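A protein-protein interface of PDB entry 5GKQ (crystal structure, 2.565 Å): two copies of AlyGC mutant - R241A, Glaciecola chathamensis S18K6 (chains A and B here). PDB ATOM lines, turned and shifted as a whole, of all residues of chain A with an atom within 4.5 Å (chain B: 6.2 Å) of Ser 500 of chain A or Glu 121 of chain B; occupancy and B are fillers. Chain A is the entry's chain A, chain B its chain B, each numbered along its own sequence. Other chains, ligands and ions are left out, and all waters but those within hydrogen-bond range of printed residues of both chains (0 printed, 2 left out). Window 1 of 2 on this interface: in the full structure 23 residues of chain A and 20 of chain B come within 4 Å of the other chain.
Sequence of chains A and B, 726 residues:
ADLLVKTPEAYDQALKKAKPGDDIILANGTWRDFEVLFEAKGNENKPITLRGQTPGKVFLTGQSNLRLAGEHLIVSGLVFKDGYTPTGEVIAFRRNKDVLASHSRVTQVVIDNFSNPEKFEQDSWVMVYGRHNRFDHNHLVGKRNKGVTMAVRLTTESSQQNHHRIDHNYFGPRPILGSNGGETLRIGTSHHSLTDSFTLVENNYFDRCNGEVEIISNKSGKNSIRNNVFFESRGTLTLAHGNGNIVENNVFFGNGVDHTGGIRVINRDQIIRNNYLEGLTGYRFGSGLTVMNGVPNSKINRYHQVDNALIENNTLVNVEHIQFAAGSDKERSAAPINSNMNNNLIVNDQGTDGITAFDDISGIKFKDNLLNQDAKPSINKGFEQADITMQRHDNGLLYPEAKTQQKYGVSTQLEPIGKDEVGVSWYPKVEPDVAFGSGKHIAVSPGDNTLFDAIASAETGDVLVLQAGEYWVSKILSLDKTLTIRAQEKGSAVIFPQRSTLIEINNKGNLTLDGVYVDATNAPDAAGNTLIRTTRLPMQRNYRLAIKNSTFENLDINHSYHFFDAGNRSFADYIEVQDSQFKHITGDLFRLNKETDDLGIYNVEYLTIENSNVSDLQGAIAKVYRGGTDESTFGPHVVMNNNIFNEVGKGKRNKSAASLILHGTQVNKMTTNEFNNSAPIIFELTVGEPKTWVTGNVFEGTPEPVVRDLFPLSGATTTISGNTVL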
ATOM      1  N   ILE A 476     -11.010  -4.345 -23.703  1.00  0.00           N
ATOM      2  CA  ILE A 476     -10.259  -5.092 -22.703  1.00  0.00           C
ATOM      3  C   ILE A 476     -10.495  -6.578 -22.925  1.00  0.00           C
ATOM      4  O   ILE A 476     -11.634  -7.021 -23.100  1.00  0.00           O
ATOM      5  CB  ILE A 476     -10.649  -4.659 -21.283  1.00  0.00           C
ATOM      6  CG1 ILE A 476      -9.974  -3.338 -20.924  1.00  0.00           C
ATOM      7  CG2 ILE A 476     -10.206  -5.680 -20.292  1.00  0.00           C
ATOM      8  CD1 ILE A 476     -10.708  -2.113 -21.398  1.00  0.00           C
ATOM      9  N   ARG A 499      -5.610   0.432 -24.788  1.00  0.00           N
ATOM     10  CA  ARG A 499      -6.340   0.748 -23.570  1.00  0.00           C
ATOM     11  C   ARG A 499      -5.400   0.680 -22.380  1.00  0.00           C
ATOM     12  O   ARG A 499      -4.327   0.088 -22.453  1.00  0.00           O
ATOM     13  CB  ARG A 499      -7.523  -0.213 -23.348  1.00  0.00           C
ATOM     14  CG  ARG A 499      -8.406  -0.372 -24.540  1.00  0.00           C
ATOM     15  CD  ARG A 499      -9.121   0.920 -24.857  1.00  0.00           C
ATOM     16  NE  ARG A 499      -9.886   1.378 -23.709  1.00  0.00           N
ATOM     17  CZ  ARG A 499     -11.037   0.838 -23.336  1.00  0.00           C
ATOM     18  NH1 ARG A 499     -11.546  -0.176 -24.018  1.00  0.00           N
ATOM     19  NH2 ARG A 499     -11.665   1.299 -22.277  1.00  0.00           N
ATOM     20  N   SER A 500      -5.826   1.277 -21.265  1.00  0.00           N
ATOM     21  CA  SER A 500      -5.003   1.228 -20.062  1.00  0.00           C
ATOM     22  C   SER A 500      -4.768  -0.196 -19.589  1.00  0.00           C
ATOM     23  O   SER A 500      -3.789  -0.441 -18.879  1.00  0.00           O
ATOM     24  CB  SER A 500      -5.624   2.054 -18.929  1.00  0.00           C
ATOM     25  OG  SER A 500      -6.996   2.279 -19.144  1.00  0.00           O
ATOM     26  N   THR A 501      -5.635  -1.131 -19.962  1.00  0.00           N
ATOM     27  CA  THR A 501      -5.443  -2.541 -19.679  1.00  0.00           C
ATOM     28  C   THR A 501      -5.586  -3.317 -20.975  1.00  0.00           C
ATOM     29  O   THR A 501      -6.480  -3.044 -21.769  1.00  0.00           O
ATOM     30  CB  THR A 501      -6.452  -3.060 -18.665  1.00  0.00           C
ATOM     31  OG1 THR A 501      -6.391  -2.264 -17.484  1.00  0.00           O
ATOM     32  CG2 THR A 501      -6.146  -4.499 -18.305  1.00  0.00           C
ATOM     33  N   LEU A 502      -4.699  -4.267 -21.202  1.00  0.00           N
ATOM     34  CA  LEU A 502      -4.887  -5.153 -22.334  1.00  0.00           C
ATOM     35  C   LEU A 502      -5.609  -6.418 -21.900  1.00  0.00           C
ATOM     36  O   LEU A 502      -6.619  -6.792 -22.488  1.00  0.00           O
ATOM     37  CB  LEU A 502      -3.540  -5.501 -22.971  1.00  0.00           C
ATOM     38  CG  LEU A 502      -3.626  -6.492 -24.132  1.00  0.00           C
ATOM     39  CD1 LEU A 502      -4.170  -5.825 -25.353  1.00  0.00           C
ATOM     40  CD2 LEU A 502      -2.284  -7.102 -24.451  1.00  0.00           C
ATOM     41  N   PRO A 524      -2.778   4.391 -23.841  1.00  0.00           N
ATOM     42  CA  PRO A 524      -3.138   5.759 -23.466  1.00  0.00           C
ATOM     43  C   PRO A 524      -1.995   6.463 -22.762  1.00  0.00           C
ATOM     44  O   PRO A 524      -1.239   5.857 -22.000  1.00  0.00           O
ATOM     45  CB  PRO A 524      -4.330   5.561 -22.532  1.00  0.00           C
ATOM     46  CG  PRO A 524      -4.819   4.210 -22.813  1.00  0.00           C
ATOM     47  CD  PRO A 524      -3.659   3.408 -23.196  1.00  0.00           C
ATOM     48  N   ASN A 529      -0.904   2.630 -16.207  1.00  0.00           N
ATOM     49  CA  ASN A 529      -1.325   1.557 -17.081  1.00  0.00           C
ATOM     50  C   ASN A 529      -0.828   0.218 -16.548  1.00  0.00           C
ATOM     51  O   ASN A 529       0.182   0.142 -15.851  1.00  0.00           O
ATOM     52  CB  ASN A 529      -0.795   1.800 -18.494  1.00  0.00           C
ATOM     53  CG  ASN A 529      -1.444   2.984 -19.160  1.00  0.00           C
ATOM     54  OD1 ASN A 529      -2.341   3.603 -18.597  1.00  0.00           O
ATOM     55  ND2 ASN A 529      -0.979   3.323 -20.355  1.00  0.00           N
ATOM     56  N   THR A 530      -1.562  -0.848 -16.876  1.00  0.00           N
ATOM     57  CA  THR A 530      -1.197  -2.216 -16.524  1.00  0.00           C
ATOM     58  C   THR A 530      -1.450  -3.078 -17.748  1.00  0.00           C
ATOM     59  O   THR A 530      -2.587  -3.169 -18.205  1.00  0.00           O
ATOM     60  CB  THR A 530      -2.025  -2.736 -15.338  1.00  0.00           C
ATOM     61  OG1 THR A 530      -3.414  -2.644 -15.668  1.00  0.00           O
ATOM     62  CG2 THR A 530      -1.778  -1.927 -14.086  1.00  0.00           C
ATOM     63  N   ARG A 533      -3.579  -7.825 -15.775  1.00  0.00           N
ATOM     64  CA  ARG A 533      -3.941  -7.654 -14.371  1.00  0.00           C
ATOM     65  C   ARG A 533      -5.097  -8.576 -14.007  1.00  0.00           C
ATOM     66  O   ARG A 533      -5.846  -9.025 -14.869  1.00  0.00           O
ATOM     67  CB  ARG A 533      -4.309  -6.200 -14.067  1.00  0.00           C
ATOM     68  CG  ARG A 533      -5.502  -5.712 -14.840  1.00  0.00           C
ATOM     69  CD  ARG A 533      -5.955  -4.345 -14.392  1.00  0.00           C
ATOM     70  NE  ARG A 533      -7.070  -3.876 -15.214  1.00  0.00           N
ATOM     71  CZ  ARG A 533      -8.345  -4.155 -14.971  1.00  0.00           C
ATOM     72  NH1 ARG A 533      -8.653  -4.888 -13.920  1.00  0.00           N
ATOM     73  NH2 ARG A 533      -9.303  -3.704 -15.771  1.00  0.00           N
ATOM     74  N   ARG A 536     -10.179  -6.035 -10.507  1.00  0.00           N
ATOM     75  CA  ARG A 536     -10.005  -5.250  -9.300  1.00  0.00           C
ATOM     76  C   ARG A 536     -11.095  -5.531  -8.285  1.00  0.00           C
ATOM     77  O   ARG A 536     -10.975  -5.112  -7.134  1.00  0.00           O
ATOM     78  CB  ARG A 536      -9.948  -3.763  -9.633  1.00  0.00           C
ATOM     79  CG  ARG A 536      -8.904  -3.456 -10.672  1.00  0.00           C
ATOM     80  CD  ARG A 536      -8.404  -2.041 -10.535  1.00  0.00           C
ATOM     81  NE  ARG A 536      -7.624  -1.621 -11.693  1.00  0.00           N
ATOM     82  CZ  ARG A 536      -8.167  -1.244 -12.851  1.00  0.00           C
ATOM     83  NH1 ARG A 536      -9.482  -1.240 -13.004  1.00  0.00           N
ATOM     84  NH2 ARG A 536      -7.386  -0.882 -13.851  1.00  0.00           N
ATOM     85  N   ASN B 116     -18.220   4.199 -17.451  1.00  0.00           N
ATOM     86  CA  ASN B 116     -17.638   2.907 -17.137  1.00  0.00           C
ATOM     87  C   ASN B 116     -17.749   2.656 -15.635  1.00  0.00           C
ATOM     88  O   ASN B 116     -17.571   3.581 -14.834  1.00  0.00           O
ATOM     89  CB  ASN B 116     -16.179   2.850 -17.586  1.00  0.00           C
ATOM     90  CG  ASN B 116     -15.595   1.455 -17.509  1.00  0.00           C
ATOM     91  OD1 ASN B 116     -15.391   0.922 -16.418  1.00  0.00           O
ATOM     92  ND2 ASN B 116     -15.294   0.867 -18.663  1.00  0.00           N
ATOM     93  N   GLU B 118     -15.782   0.876 -13.686  1.00  0.00           N
ATOM     94  CA  GLU B 118     -14.504   0.999 -13.003  1.00  0.00           C
ATOM     95  C   GLU B 118     -14.002   2.424 -13.161  1.00  0.00           C
ATOM     96  O   GLU B 118     -13.637   2.838 -14.263  1.00  0.00           O
ATOM     97  CB  GLU B 118     -13.502  -0.005 -13.540  1.00  0.00           C
ATOM     98  CG  GLU B 118     -13.139  -1.000 -12.485  1.00  0.00           C
ATOM     99  CD  GLU B 118     -12.263  -2.076 -13.012  1.00  0.00           C
ATOM    100  OE1 GLU B 118     -11.416  -2.551 -12.235  1.00  0.00           O
ATOM    101  OE2 GLU B 118     -12.404  -2.430 -14.206  1.00  0.00           O
ATOM    102  N   LYS B 119     -13.970   3.165 -12.051  1.00  0.00           N
ATOM    103  CA  LYS B 119     -13.695   4.596 -12.095  1.00  0.00           C
ATOM    104  C   LYS B 119     -12.383   4.931 -12.776  1.00  0.00           C
ATOM    105  O   LYS B 119     -12.214   6.066 -13.217  1.00  0.00           O
ATOM    106  CB  LYS B 119     -13.704   5.171 -10.679  1.00  0.00           C
ATOM    107  CG  LYS B 119     -13.548   6.672 -10.601  1.00  0.00           C
ATOM    108  CD  LYS B 119     -14.062   7.224  -9.292  1.00  0.00           C
ATOM    109  CE  LYS B 119     -13.336   8.511  -8.923  1.00  0.00           C
ATOM    110  NZ  LYS B 119     -14.251   9.674  -8.675  1.00  0.00           N
ATOM    111  N   PHE B 120     -11.464   3.976 -12.909  1.00  0.00           N
ATOM    112  CA  PHE B 120     -10.151   4.267 -13.468  1.00  0.00           C
ATOM    113  C   PHE B 120      -9.770   3.308 -14.576  1.00  0.00           C
ATOM    114  O   PHE B 120      -8.592   3.047 -14.786  1.00  0.00           O
ATOM    115  CB  PHE B 120      -9.073   4.271 -12.390  1.00  0.00           C
ATOM    116  CG  PHE B 120      -9.190   5.422 -11.461  1.00  0.00           C
ATOM    117  CD1 PHE B 120      -8.736   6.664 -11.836  1.00  0.00           C
ATOM    118  CD2 PHE B 120      -9.803   5.274 -10.233  1.00  0.00           C
ATOM    119  CE1 PHE B 120      -8.867   7.733 -10.995  1.00  0.00           C
ATOM    120  CE2 PHE B 120      -9.937   6.338  -9.384  1.00  0.00           C
ATOM    121  CZ  PHE B 120      -9.471   7.568  -9.761  1.00  0.00           C
ATOM    122  N   GLU B 121     -10.739   2.760 -15.285  1.00  0.00           N
ATOM    123  CA  GLU B 121     -10.487   2.360 -16.655  1.00  0.00           C
ATOM    124  C   GLU B 121     -10.878   3.557 -17.504  1.00  0.00           C
ATOM    125  O   GLU B 121     -11.949   4.142 -17.308  1.00  0.00           O
ATOM    126  CB  GLU B 121     -11.272   1.117 -17.056  1.00  0.00           C
ATOM    127  CG  GLU B 121     -10.799   0.492 -18.372  1.00  0.00           C
ATOM    128  CD  GLU B 121      -9.482  -0.252 -18.243  1.00  0.00           C
ATOM    129  OE1 GLU B 121      -9.261  -0.895 -17.204  1.00  0.00           O
ATOM    130  OE2 GLU B 121      -8.675  -0.217 -19.189  1.00  0.00           O
ATOM    131  N   GLN B 122      -9.995   3.953 -18.403  1.00  0.00           N
ATOM    132  CA  GLN B 122     -10.112   5.242 -19.055  1.00  0.00           C
ATOM    133  C   GLN B 122     -10.786   5.112 -20.414  1.00  0.00           C
ATOM    134  O   GLN B 122     -10.490   4.195 -21.188  1.00  0.00           O
ATOM    135  CB  GLN B 122      -8.735   5.880 -19.221  1.00  0.00           C
ATOM    136  CG  GLN B 122      -8.624   6.810 -20.410  1.00  0.00           C
ATOM    137  CD  GLN B 122      -7.430   7.712 -20.315  1.00  0.00           C
ATOM    138  OE1 GLN B 122      -6.890   7.916 -19.249  1.00  0.00           O
ATOM    139  NE2 GLN B 122      -7.028   8.260 -21.420  1.00  0.00           N
ATOM    140  N   ASP B 123     -11.673   6.056 -20.705  1.00  0.00           N
ATOM    141  CA  ASP B 123     -12.248   6.189 -22.028  1.00  0.00           C
ATOM    142  C   ASP B 123     -12.588   7.648 -22.247  1.00  0.00           C
ATOM    143  O   ASP B 123     -12.464   8.478 -21.350  1.00  0.00           O
ATOM    144  CB  ASP B 123     -13.498   5.312 -22.211  1.00  0.00           C
ATOM    145  CG  ASP B 123     -14.676   5.741 -21.324  1.00  0.00           C
ATOM    146  OD1 ASP B 123     -14.650   6.813 -20.695  1.00  0.00           O
ATOM    147  OD2 ASP B 123     -15.662   4.981 -21.259  1.00  0.00           O
ATOM    148  N   ASN B 145     -15.773   8.603 -14.826  1.00  0.00           N
ATOM    149  CA  ASN B 145     -14.565   7.805 -14.896  1.00  0.00           C
ATOM    150  C   ASN B 145     -13.425   8.615 -15.499  1.00  0.00           C
ATOM    151  O   ASN B 145     -13.606   9.714 -16.025  1.00  0.00           O
ATOM    152  CB  ASN B 145     -14.802   6.525 -15.699  1.00  0.00           C
ATOM    153  CG  ASN B 145     -14.934   6.784 -17.170  1.00  0.00           C
ATOM    154  OD1 ASN B 145     -15.518   7.777 -17.582  1.00  0.00           O
ATOM    155  ND2 ASN B 145     -14.410   5.879 -17.978  1.00  0.00           N
ATOM    156  N   LYS B 146     -12.233   8.045 -15.405  1.00  0.00           N
ATOM    157  CA  LYS B 146     -11.043   8.706 -15.908  1.00  0.00           C
ATOM    158  C   LYS B 146     -11.125   8.914 -17.411  1.00  0.00           C
ATOM    159  O   LYS B 146     -11.567   8.034 -18.154  1.00  0.00           O
ATOM    160  CB  LYS B 146      -9.823   7.864 -15.602  1.00  0.00           C
ATOM    161  CG  LYS B 146      -8.661   8.238 -16.444  1.00  0.00           C
ATOM    162  CD  LYS B 146      -7.799   9.320 -15.820  1.00  0.00           C
ATOM    163  CE  LYS B 146      -6.743   8.822 -14.903  1.00  0.00           C
ATOM    164  NZ  LYS B 146      -5.803   7.935 -15.578  1.00  0.00           N
ATOM    165  N   GLY B 147     -10.640  10.063 -17.868  1.00  0.00           N
ATOM    166  CA  GLY B 147     -10.632  10.254 -19.303  1.00  0.00           C
ATOM    167  C   GLY B 147     -11.420  11.490 -19.684  1.00  0.00           C
ATOM    168  O   GLY B 147     -12.518  11.742 -19.186  1.00  0.00           O
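No position is printed for both chains.
The side-chain carboxylate of Glu 121 of chain B lies within salt-bridge range of the guanidinium group of Arg 533 of chain A, 3.2 Å away. The side-chain carboxylate of Glu 118 of chain B lies within salt-bridge range of the guanidinium group of Arg 533 of chain A, 3.7 Å away. The guanidinium group (NH2) of Arg 499 of chain A is in hydrogen-bond range of the backbone carbonyl oxygen (O) of Gln 122 of chain B. The guanidinium group of Arg 536 of chain A lies within salt-bridge range of the side-chain carboxylate of Glu 121 of chain B, at 3.8 Å. NH1 of Arg 536 of chain A is in salt-bridge range of OE1 of Glu 118 of chain B (2.5 Å). The side-chain hydroxyl (OG1) of Thr 501 of chain A is in hydrogen-bond range of the side-chain carboxylate (OE1) of Glu 121 of chain B. The side-chain hydroxyl (OG) of Ser 500 of chain A is in hydrogen-bond range of the side-chain carboxylate (OE2) of Glu 121 of chain B (3.0 Å).
CD1 of Ile 476 of chain A touches OE2 of Glu 121 of chain B, at 3.6 Å. N of Gln 122 of chain B touches OG of Ser 500 of chain A (3.5 Å). CB of Pro 524 of chain A touches NE2 of Gln 122 of chain B, 3.97 Å away.
Among the printed residues, Asp or Glu carboxylates within 4 Å of a Lys or Arg side-chain nitrogen of the other chain: Arg 533 of chain A with Glu 118 of chain B, Arg 533 of chain A with Glu 121 of chain B, Arg 536 of chain A with Glu 118 of chain B and Arg 536 of chain A with Glu 121 of chain B.
Of the printed residues of chain B, Ile 476 of chain A touches Glu 121 (3.6 Å). Ser 500 of chain A touches just these residues of chain B: Glu 121 and Gln 122. Thr 530 of chain A touches none of the printed residues of chain B. Of the printed residues of chain A, Glu 118 of chain B touches Arg 533 and Arg 536. Printed residues of chain A within 4 Å of Glu 121 of chain B: Ile 476 (3.6 Å), Ser 500 (3.0 Å), Thr 501 (3.2 Å), Arg 533 (3.2 Å) and Arg 536 (3.8 Å). Lys 146 of chain B touches none of the printed residues of chain A.
OG1 of Thr 501 of chain A lies within hydrogen-bond range of NE of Arg 533 of chain A. The backbone carbonyl oxygen of Pro 524 of chain A sits at hydrogen-bond distance from the side-chain amide nitrogen of Asn 529 of chain A (3.0 Å). The backbone NH of Thr 530 of chain A lies within hydrogen-bond range of the backbone carbonyl oxygen of Ser 500 of chain A (3.0 Å). OD1 of Asn 116 of chain B sits at hydrogen-bond distance from N of Glu 118 of chain B. O of Glu 121 of chain B is in hydrogen-bond range of ND2 of Asn 145 of chain B (3.1 Å).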
